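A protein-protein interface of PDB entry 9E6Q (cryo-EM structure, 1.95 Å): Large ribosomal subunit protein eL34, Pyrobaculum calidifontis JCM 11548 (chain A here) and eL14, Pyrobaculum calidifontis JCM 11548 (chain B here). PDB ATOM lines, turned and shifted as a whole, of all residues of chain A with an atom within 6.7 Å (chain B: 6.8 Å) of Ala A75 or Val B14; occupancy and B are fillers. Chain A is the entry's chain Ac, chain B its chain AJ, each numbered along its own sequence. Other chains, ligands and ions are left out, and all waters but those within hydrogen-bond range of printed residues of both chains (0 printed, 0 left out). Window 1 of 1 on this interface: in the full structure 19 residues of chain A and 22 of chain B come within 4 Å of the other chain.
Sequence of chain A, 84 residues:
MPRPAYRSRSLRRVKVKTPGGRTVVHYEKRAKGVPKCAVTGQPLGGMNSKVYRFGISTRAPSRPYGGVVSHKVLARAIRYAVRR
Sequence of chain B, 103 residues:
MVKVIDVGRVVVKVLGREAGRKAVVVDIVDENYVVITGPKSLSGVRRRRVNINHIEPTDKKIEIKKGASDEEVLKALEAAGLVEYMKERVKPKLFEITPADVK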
ATOM      1  N   ARG A  63       0.835  -1.905 -17.658  1.00  0.00           N
ATOM      2  CA  ARG A  63       0.499  -3.111 -18.394  1.00  0.00           C
ATOM      3  C   ARG A  63       0.206  -4.197 -17.384  1.00  0.00           C
ATOM      4  O   ARG A  63       0.782  -4.185 -16.293  1.00  0.00           O
ATOM      5  CB  ARG A  63       1.646  -3.541 -19.316  1.00  0.00           C
ATOM      6  CG  ARG A  63       1.198  -4.273 -20.554  1.00  0.00           C
ATOM      7  CD  ARG A  63       2.350  -4.628 -21.457  1.00  0.00           C
ATOM      8  NE  ARG A  63       3.620  -4.661 -20.751  1.00  0.00           N
ATOM      9  CZ  ARG A  63       4.616  -3.818 -20.976  1.00  0.00           C
ATOM     10  NH1 ARG A  63       4.513  -2.852 -21.869  1.00  0.00           N
ATOM     11  NH2 ARG A  63       5.741  -3.945 -20.283  1.00  0.00           N
ATOM     12  N   SER A  70       8.440  -9.056 -19.690  1.00  0.00           N
ATOM     13  CA  SER A  70       8.469  -8.098 -20.777  1.00  0.00           C
ATOM     14  C   SER A  70       7.165  -8.146 -21.558  1.00  0.00           C
ATOM     15  O   SER A  70       6.361  -9.067 -21.421  1.00  0.00           O
ATOM     16  CB  SER A  70       9.651  -8.378 -21.701  1.00  0.00           C
ATOM     17  OG  SER A  70       9.562  -9.673 -22.257  1.00  0.00           O
ATOM     18  N   HIS A  71       6.954  -7.117 -22.377  1.00  0.00           N
ATOM     19  CA  HIS A  71       5.763  -7.065 -23.213  1.00  0.00           C
ATOM     20  C   HIS A  71       5.703  -8.254 -24.162  1.00  0.00           C
ATOM     21  O   HIS A  71       4.619  -8.757 -24.466  1.00  0.00           O
ATOM     22  CB  HIS A  71       5.745  -5.756 -23.997  1.00  0.00           C
ATOM     23  CG  HIS A  71       6.733  -5.722 -25.120  1.00  0.00           C
ATOM     24  ND1 HIS A  71       8.068  -5.454 -24.929  1.00  0.00           N
ATOM     25  CD2 HIS A  71       6.583  -5.960 -26.442  1.00  0.00           C
ATOM     26  CE1 HIS A  71       8.697  -5.508 -26.087  1.00  0.00           C
ATOM     27  NE2 HIS A  71       7.817  -5.814 -27.022  1.00  0.00           N
ATOM     28  N   LYS A  72       6.860  -8.712 -24.642  1.00  0.00           N
ATOM     29  CA  LYS A  72       6.892  -9.834 -25.574  1.00  0.00           C
ATOM     30  C   LYS A  72       6.371 -11.107 -24.928  1.00  0.00           C
ATOM     31  O   LYS A  72       5.628 -11.870 -25.552  1.00  0.00           O
ATOM     32  CB  LYS A  72       8.314 -10.045 -26.084  1.00  0.00           C
ATOM     33  CG  LYS A  72       8.537  -9.636 -27.518  1.00  0.00           C
ATOM     34  CD  LYS A  72       9.938  -9.997 -27.967  1.00  0.00           C
ATOM     35  CE  LYS A  72      10.667  -8.793 -28.521  1.00  0.00           C
ATOM     36  NZ  LYS A  72      11.803  -9.178 -29.394  1.00  0.00           N
ATOM     37  N   VAL A  73       6.770 -11.364 -23.684  1.00  0.00           N
ATOM     38  CA  VAL A  73       6.302 -12.548 -22.978  1.00  0.00           C
ATOM     39  C   VAL A  73       4.811 -12.450 -22.698  1.00  0.00           C
ATOM     40  O   VAL A  73       4.080 -13.436 -22.820  1.00  0.00           O
ATOM     41  CB  VAL A  73       7.115 -12.745 -21.687  1.00  0.00           C
ATOM     42  CG1 VAL A  73       6.499 -13.821 -20.826  1.00  0.00           C
ATOM     43  CG2 VAL A  73       8.550 -13.088 -22.023  1.00  0.00           C
ATOM     44  N   LEU A  74       4.334 -11.269 -22.310  1.00  0.00           N
ATOM     45  CA  LEU A  74       2.921 -11.118 -21.981  1.00  0.00           C
ATOM     46  C   LEU A  74       2.042 -11.323 -23.205  1.00  0.00           C
ATOM     47  O   LEU A  74       1.029 -12.025 -23.139  1.00  0.00           O
ATOM     48  CB  LEU A  74       2.657  -9.746 -21.372  1.00  0.00           C
ATOM     49  CG  LEU A  74       1.182  -9.581 -21.009  1.00  0.00           C
ATOM     50  CD1 LEU A  74       0.805 -10.521 -19.882  1.00  0.00           C
ATOM     51  CD2 LEU A  74       0.837  -8.155 -20.654  1.00  0.00           C
ATOM     52  N   ALA A  75       2.411 -10.711 -24.331  1.00  0.00           N
ATOM     53  CA  ALA A  75       1.598 -10.825 -25.536  1.00  0.00           C
ATOM     54  C   ALA A  75       1.513 -12.267 -26.010  1.00  0.00           C
ATOM     55  O   ALA A  75       0.434 -12.746 -26.366  1.00  0.00           O
ATOM     56  CB  ALA A  75       2.163  -9.938 -26.639  1.00  0.00           C
ATOM     57  N   ARG A  76       2.639 -12.977 -26.012  1.00  0.00           N
ATOM     58  CA  ARG A  76       2.632 -14.369 -26.439  1.00  0.00           C
ATOM     59  C   ARG A  76       1.795 -15.229 -25.501  1.00  0.00           C
ATOM     60  O   ARG A  76       1.044 -16.098 -25.951  1.00  0.00           O
ATOM     61  CB  ARG A  76       4.064 -14.885 -26.528  1.00  0.00           C
ATOM     62  CG  ARG A  76       4.204 -16.389 -26.539  1.00  0.00           C
ATOM     63  CD  ARG A  76       3.798 -17.000 -27.863  1.00  0.00           C
ATOM     64  NE  ARG A  76       3.850 -16.053 -28.967  1.00  0.00           N
ATOM     65  CZ  ARG A  76       3.197 -16.207 -30.110  1.00  0.00           C
ATOM     66  NH1 ARG A  76       2.441 -17.266 -30.335  1.00  0.00           N
ATOM     67  NH2 ARG A  76       3.305 -15.274 -31.049  1.00  0.00           N
ATOM     68  N   ALA A  77       1.896 -14.990 -24.194  1.00  0.00           N
ATOM     69  CA  ALA A  77       1.130 -15.780 -23.240  1.00  0.00           C
ATOM     70  C   ALA A  77      -0.362 -15.510 -23.365  1.00  0.00           C
ATOM     71  O   ALA A  77      -1.178 -16.412 -23.159  1.00  0.00           O
ATOM     72  CB  ALA A  77       1.614 -15.503 -21.822  1.00  0.00           C
ATOM     73  N   ILE A  78      -0.741 -14.275 -23.687  1.00  0.00           N
ATOM     74  CA  ILE A  78      -2.150 -13.968 -23.897  1.00  0.00           C
ATOM     75  C   ILE A  78      -2.657 -14.624 -25.173  1.00  0.00           C
ATOM     76  O   ILE A  78      -3.779 -15.137 -25.217  1.00  0.00           O
ATOM     77  CB  ILE A  78      -2.366 -12.445 -23.910  1.00  0.00           C
ATOM     78  CG1 ILE A  78      -2.202 -11.881 -22.505  1.00  0.00           C
ATOM     79  CG2 ILE A  78      -3.734 -12.101 -24.442  1.00  0.00           C
ATOM     80  CD1 ILE A  78      -2.352 -10.389 -22.437  1.00  0.00           C
ATOM     81  N   ARG A  79      -1.841 -14.629 -26.228  1.00  0.00           N
ATOM     82  CA  ARG A  79      -2.237 -15.300 -27.461  1.00  0.00           C
ATOM     83  C   ARG A  79      -2.470 -16.786 -27.229  1.00  0.00           C
ATOM     84  O   ARG A  79      -3.406 -17.366 -27.786  1.00  0.00           O
ATOM     85  CB  ARG A  79      -1.174 -15.094 -28.537  1.00  0.00           C
ATOM     86  CG  ARG A  79      -1.237 -13.751 -29.207  1.00  0.00           C
ATOM     87  CD  ARG A  79      -0.278 -13.679 -30.365  1.00  0.00           C
ATOM     88  NE  ARG A  79       0.284 -12.345 -30.514  1.00  0.00           N
ATOM     89  CZ  ARG A  79      -0.272 -11.378 -31.226  1.00  0.00           C
ATOM     90  NH1 ARG A  79      -1.408 -11.564 -31.873  1.00  0.00           N
ATOM     91  NH2 ARG A  79       0.322 -10.193 -31.286  1.00  0.00           N
ATOM     92  N   TYR A  80      -1.627 -17.418 -26.415  1.00  0.00           N
ATOM     93  CA  TYR A  80      -1.820 -18.829 -26.108  1.00  0.00           C
ATOM     94  C   TYR A  80      -3.119 -19.058 -25.350  1.00  0.00           C
ATOM     95  O   TYR A  80      -3.820 -20.042 -25.597  1.00  0.00           O
ATOM     96  CB  TYR A  80      -0.645 -19.364 -25.298  1.00  0.00           C
ATOM     97  CG  TYR A  80       0.580 -19.694 -26.108  1.00  0.00           C
ATOM     98  CD1 TYR A  80       0.508 -19.865 -27.480  1.00  0.00           C
ATOM     99  CD2 TYR A  80       1.811 -19.841 -25.497  1.00  0.00           C
ATOM    100  CE1 TYR A  80       1.635 -20.170 -28.218  1.00  0.00           C
ATOM    101  CE2 TYR A  80       2.937 -20.144 -26.224  1.00  0.00           C
ATOM    102  CZ  TYR A  80       2.843 -20.310 -27.582  1.00  0.00           C
ATOM    103  OH  TYR A  80       3.972 -20.611 -28.295  1.00  0.00           O
ATOM    104  N   VAL A  82      -5.923 -17.163 -25.216  1.00  0.00           N
ATOM    105  CA  VAL A  82      -7.126 -16.867 -25.988  1.00  0.00           C
ATOM    106  C   VAL A  82      -7.553 -18.084 -26.795  1.00  0.00           C
ATOM    107  O   VAL A  82      -8.741 -18.415 -26.871  1.00  0.00           O
ATOM    108  CB  VAL A  82      -6.881 -15.643 -26.888  1.00  0.00           C
ATOM    109  CG1 VAL A  82      -7.852 -15.619 -28.050  1.00  0.00           C
ATOM    110  CG2 VAL A  82      -6.983 -14.374 -26.079  1.00  0.00           C
ATOM    111  N   VAL B  12      -9.016  -9.763 -28.608  1.00  0.00           N
ATOM    112  CA  VAL B  12      -8.416  -9.526 -27.302  1.00  0.00           C
ATOM    113  C   VAL B  12      -7.122  -8.762 -27.524  1.00  0.00           C
ATOM    114  O   VAL B  12      -6.217  -9.258 -28.205  1.00  0.00           O
ATOM    115  CB  VAL B  12      -8.147 -10.840 -26.553  1.00  0.00           C
ATOM    116  CG1 VAL B  12      -7.419 -10.567 -25.258  1.00  0.00           C
ATOM    117  CG2 VAL B  12      -9.439 -11.579 -26.296  1.00  0.00           C
ATOM    118  N   LYS B  13      -7.029  -7.564 -26.961  1.00  0.00           N
ATOM    119  CA  LYS B  13      -5.804  -6.790 -27.085  1.00  0.00           C
ATOM    120  C   LYS B  13      -4.675  -7.455 -26.308  1.00  0.00           C
ATOM    121  O   LYS B  13      -4.868  -7.923 -25.184  1.00  0.00           O
ATOM    122  CB  LYS B  13      -6.017  -5.363 -26.593  1.00  0.00           C
ATOM    123  CG  LYS B  13      -4.963  -4.405 -27.097  1.00  0.00           C
ATOM    124  CD  LYS B  13      -5.390  -2.967 -26.973  1.00  0.00           C
ATOM    125  CE  LYS B  13      -4.315  -2.048 -27.508  1.00  0.00           C
ATOM    126  NZ  LYS B  13      -4.866  -0.776 -28.011  1.00  0.00           N
ATOM    127  N   VAL B  14      -3.490  -7.501 -26.915  1.00  0.00           N
ATOM    128  CA  VAL B  14      -2.368  -8.216 -26.319  1.00  0.00           C
ATOM    129  C   VAL B  14      -1.282  -7.298 -25.765  1.00  0.00           C
ATOM    130  O   VAL B  14      -0.455  -7.758 -24.965  1.00  0.00           O
ATOM    131  CB  VAL B  14      -1.744  -9.207 -27.323  1.00  0.00           C
ATOM    132  CG1 VAL B  14      -2.755 -10.254 -27.735  1.00  0.00           C
ATOM    133  CG2 VAL B  14      -1.201  -8.474 -28.529  1.00  0.00           C
ATOM    134  N   LEU B  15      -1.257  -6.026 -26.154  1.00  0.00           N
ATOM    135  CA  LEU B  15      -0.262  -5.086 -25.659  1.00  0.00           C
ATOM    136  C   LEU B  15      -0.946  -3.834 -25.137  1.00  0.00           C
ATOM    137  O   LEU B  15      -2.142  -3.622 -25.327  1.00  0.00           O
ATOM    138  CB  LEU B  15       0.751  -4.698 -26.743  1.00  0.00           C
ATOM    139  CG  LEU B  15       1.789  -5.735 -27.152  1.00  0.00           C
ATOM    140  CD1 LEU B  15       2.666  -5.188 -28.253  1.00  0.00           C
ATOM    141  CD2 LEU B  15       2.623  -6.140 -25.961  1.00  0.00           C
ATOM    142  N   GLY B  16      -0.158  -2.995 -24.483  1.00  0.00           N
ATOM    143  CA  GLY B  16      -0.651  -1.743 -23.959  1.00  0.00           C
ATOM    144  C   GLY B  16      -1.280  -1.900 -22.595  1.00  0.00           C
ATOM    145  O   GLY B  16      -1.302  -2.970 -21.992  1.00  0.00           O
ATOM    146  N   GLU B  18      -4.391  -1.750 -21.961  1.00  0.00           N
ATOM    147  CA  GLU B  18      -5.618  -2.517 -22.094  1.00  0.00           C
ATOM    148  C   GLU B  18      -5.377  -3.962 -22.500  1.00  0.00           C
ATOM    149  O   GLU B  18      -6.317  -4.631 -22.932  1.00  0.00           O
ATOM    150  CB  GLU B  18      -6.529  -1.847 -23.113  1.00  0.00           C
ATOM    151  CG  GLU B  18      -7.283  -0.672 -22.563  1.00  0.00           C
ATOM    152  CD  GLU B  18      -7.666   0.310 -23.638  1.00  0.00           C
ATOM    153  OE1 GLU B  18      -8.543   1.159 -23.390  1.00  0.00           O
ATOM    154  OE2 GLU B  18      -7.087   0.236 -24.738  1.00  0.00           O
ATOM    155  N   ALA B  19      -4.148  -4.454 -22.383  1.00  0.00           N
ATOM    156  CA  ALA B  19      -3.860  -5.829 -22.762  1.00  0.00           C
ATOM    157  C   ALA B  19      -4.684  -6.799 -21.927  1.00  0.00           C
ATOM    158  O   ALA B  19      -4.889  -6.599 -20.730  1.00  0.00           O
ATOM    159  CB  ALA B  19      -2.373  -6.124 -22.593  1.00  0.00           C
ATOM    160  N   GLY B  20      -5.158  -7.858 -22.574  1.00  0.00           N
ATOM    161  CA  GLY B  20      -5.944  -8.872 -21.916  1.00  0.00           C
ATOM    162  C   GLY B  20      -7.431  -8.619 -21.897  1.00  0.00           C
ATOM    163  O   GLY B  20      -8.178  -9.471 -21.404  1.00  0.00           O
ATOM    164  N   ARG B  21      -7.887  -7.487 -22.417  1.00  0.00           N
ATOM    165  CA  ARG B  21      -9.296  -7.130 -22.401  1.00  0.00           C
ATOM    166  C   ARG B  21      -9.921  -7.372 -23.767  1.00  0.00           C
ATOM    167  O   ARG B  21      -9.304  -7.111 -24.802  1.00  0.00           O
ATOM    168  CB  ARG B  21      -9.481  -5.668 -21.995  1.00  0.00           C
ATOM    169  CG  ARG B  21      -8.947  -5.327 -20.622  1.00  0.00           C
ATOM    170  CD  ARG B  21      -9.097  -3.849 -20.327  1.00  0.00           C
ATOM    171  NE  ARG B  21      -8.557  -3.487 -19.023  1.00  0.00           N
ATOM    172  CZ  ARG B  21      -9.151  -3.743 -17.866  1.00  0.00           C
ATOM    173  NH1 ARG B  21     -10.332  -4.335 -17.807  1.00  0.00           N
ATOM    174  NH2 ARG B  21      -8.546  -3.390 -16.735  1.00  0.00           N
ATOM    175  N   ASN B  53      -1.420  -6.062 -35.325  1.00  0.00           N
ATOM    176  CA  ASN B  53      -0.468  -6.923 -34.643  1.00  0.00           C
ATOM    177  C   ASN B  53      -0.651  -6.917 -33.135  1.00  0.00           C
ATOM    178  O   ASN B  53      -0.100  -7.786 -32.457  1.00  0.00           O
ATOM    179  CB  ASN B  53       0.956  -6.500 -34.984  1.00  0.00           C
ATOM    180  CG  ASN B  53       1.265  -6.661 -36.445  1.00  0.00           C
ATOM    181  OD1 ASN B  53       0.860  -7.636 -37.070  1.00  0.00           O
ATOM    182  ND2 ASN B  53       1.968  -5.689 -37.011  1.00  0.00           N
ATOM    183  N   HIS B  54      -1.410  -5.968 -32.595  1.00  0.00           N
ATOM    184  CA  HIS B  54      -1.596  -5.860 -31.157  1.00  0.00           C
ATOM    185  C   HIS B  54      -2.944  -6.388 -30.691  1.00  0.00           C
ATOM    186  O   HIS B  54      -3.325  -6.150 -29.544  1.00  0.00           O
ATOM    187  CB  HIS B  54      -1.408  -4.413 -30.711  1.00  0.00           C
ATOM    188  CG  HIS B  54      -0.104  -3.822 -31.137  1.00  0.00           C
ATOM    189  ND1 HIS B  54       0.052  -2.486 -31.420  1.00  0.00           N
ATOM    190  CD2 HIS B  54       1.104  -4.393 -31.344  1.00  0.00           C
ATOM    191  CE1 HIS B  54       1.303  -2.256 -31.772  1.00  0.00           C
ATOM    192  NE2 HIS B  54       1.963  -3.397 -31.733  1.00  0.00           N
ATOM    193  N   ILE B  55      -3.671  -7.100 -31.545  1.00  0.00           N
ATOM    194  CA  ILE B  55      -4.906  -7.766 -31.157  1.00  0.00           C
ATOM    195  C   ILE B  55      -4.839  -9.208 -31.625  1.00  0.00           C
ATOM    196  O   ILE B  55      -4.321  -9.495 -32.708  1.00  0.00           O
ATOM    197  CB  ILE B  55      -6.156  -7.073 -31.735  1.00  0.00           C
ATOM    198  CG1 ILE B  55      -5.955  -6.760 -33.215  1.00  0.00           C
ATOM    199  CG2 ILE B  55      -6.495  -5.827 -30.932  1.00  0.00           C
ATOM    200  CD1 ILE B  55      -7.196  -6.303 -33.910  1.00  0.00           C
ATOM    201  N   GLU B  56      -5.339 -10.117 -30.795  1.00  0.00           N
ATOM    202  CA  GLU B  56      -5.459 -11.511 -31.180  1.00  0.00           C
ATOM    203  C   GLU B  56      -6.915 -11.814 -31.476  1.00  0.00           C
ATOM    204  O   GLU B  56      -7.772 -11.566 -30.615  1.00  0.00           O
ATOM    205  CB  GLU B  56      -4.939 -12.424 -30.080  1.00  0.00           C
ATOM    206  CG  GLU B  56      -5.221 -13.895 -30.302  1.00  0.00           C
ATOM    207  CD  GLU B  56      -4.151 -14.595 -31.118  1.00  0.00           C
ATOM    208  OE1 GLU B  56      -3.346 -13.907 -31.777  1.00  0.00           O
ATOM    209  OE2 GLU B  56      -4.113 -15.842 -31.104  1.00  0.00           O
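The backbone carbonyl oxygen (O) of Val B12 lies within hydrogen-bond range of the backbone NH (N) of Glu B56 (2.9 Å). N of Gly B20 sits at hydrogen-bond distance from O of Lys B13, at 2.6 Å. The backbone NH (N) of Val B14 sits at hydrogen-bond distance from the backbone carbonyl oxygen (O) of His B54 (3.0 Å).
Hydrophobic or aromatic side chains of chain B within 4 Å of the printed part of chain A: Val B12, Val B14 and Leu B15. Among the printed residues, 12 pairs touch across the chains. Among the printed residues, Asp or Glu carboxylates within 4 Å of a Lys or Arg side-chain nitrogen of the other chain: Arg A79 with Glu B56 (3.0 Å).
Printed residues of chain B within 4 Å of Arg A63: Gly B16. Ala A75 touches just these residues of chain B: Val B14 (3.7 Å) and Leu B15 (3.9 Å). Of the printed residues of chain B, Ile A78 touches Val B14 (3.9 Å) and Gly B20 (3.8 Å). Printed residues of chain B within 4 Å of Val A82: Val B12 (3.7 Å) and Glu B56 (3.9 Å). Val B14 touches just these residues of chain A: Ala A75 (3.7 Å), Ile A78 (3.9 Å) and Arg A79 (3.6 Å). Glu B18 touches none of the printed residues of chain A. Printed residues of chain A within 4 Å of Glu B56: Arg A79 and Val A82. The nearest residue of chain B that does not touch Ala A75 is Glu B56 (6.5 Å). The nearest residue of chain A that does not touch Val B14 is Leu A74 (4.5 Å).
Among the printed residues, pairs that only touch across the chains: Arg A63 with Gly B16 (3.2 Å), Arg A79 with Val B14 (3.6 Å), His A71 with Leu B15 (3.6 Å), Arg A79 with Ile B55 (3.7 Å), Val A82 with Val B12 (3.7 Å), Ala A75 with Val B14 (3.7 Å), Ile A78 with Gly B20 (3.8 Å), Val A82 with Glu B56 (3.9 Å), Ala A75 with Leu B15 (3.9 Å) and Ile A78 with Val B14 (3.9 Å).
The backbone carbonyl oxygen (O) of Asn B53 lies within hydrogen-bond range of the guanidinium group (NH2) of Arg A79, 2.7 Å away. The side-chain carboxylate of Glu B56 lies within salt-bridge range of the guanidinium group of Arg A79.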
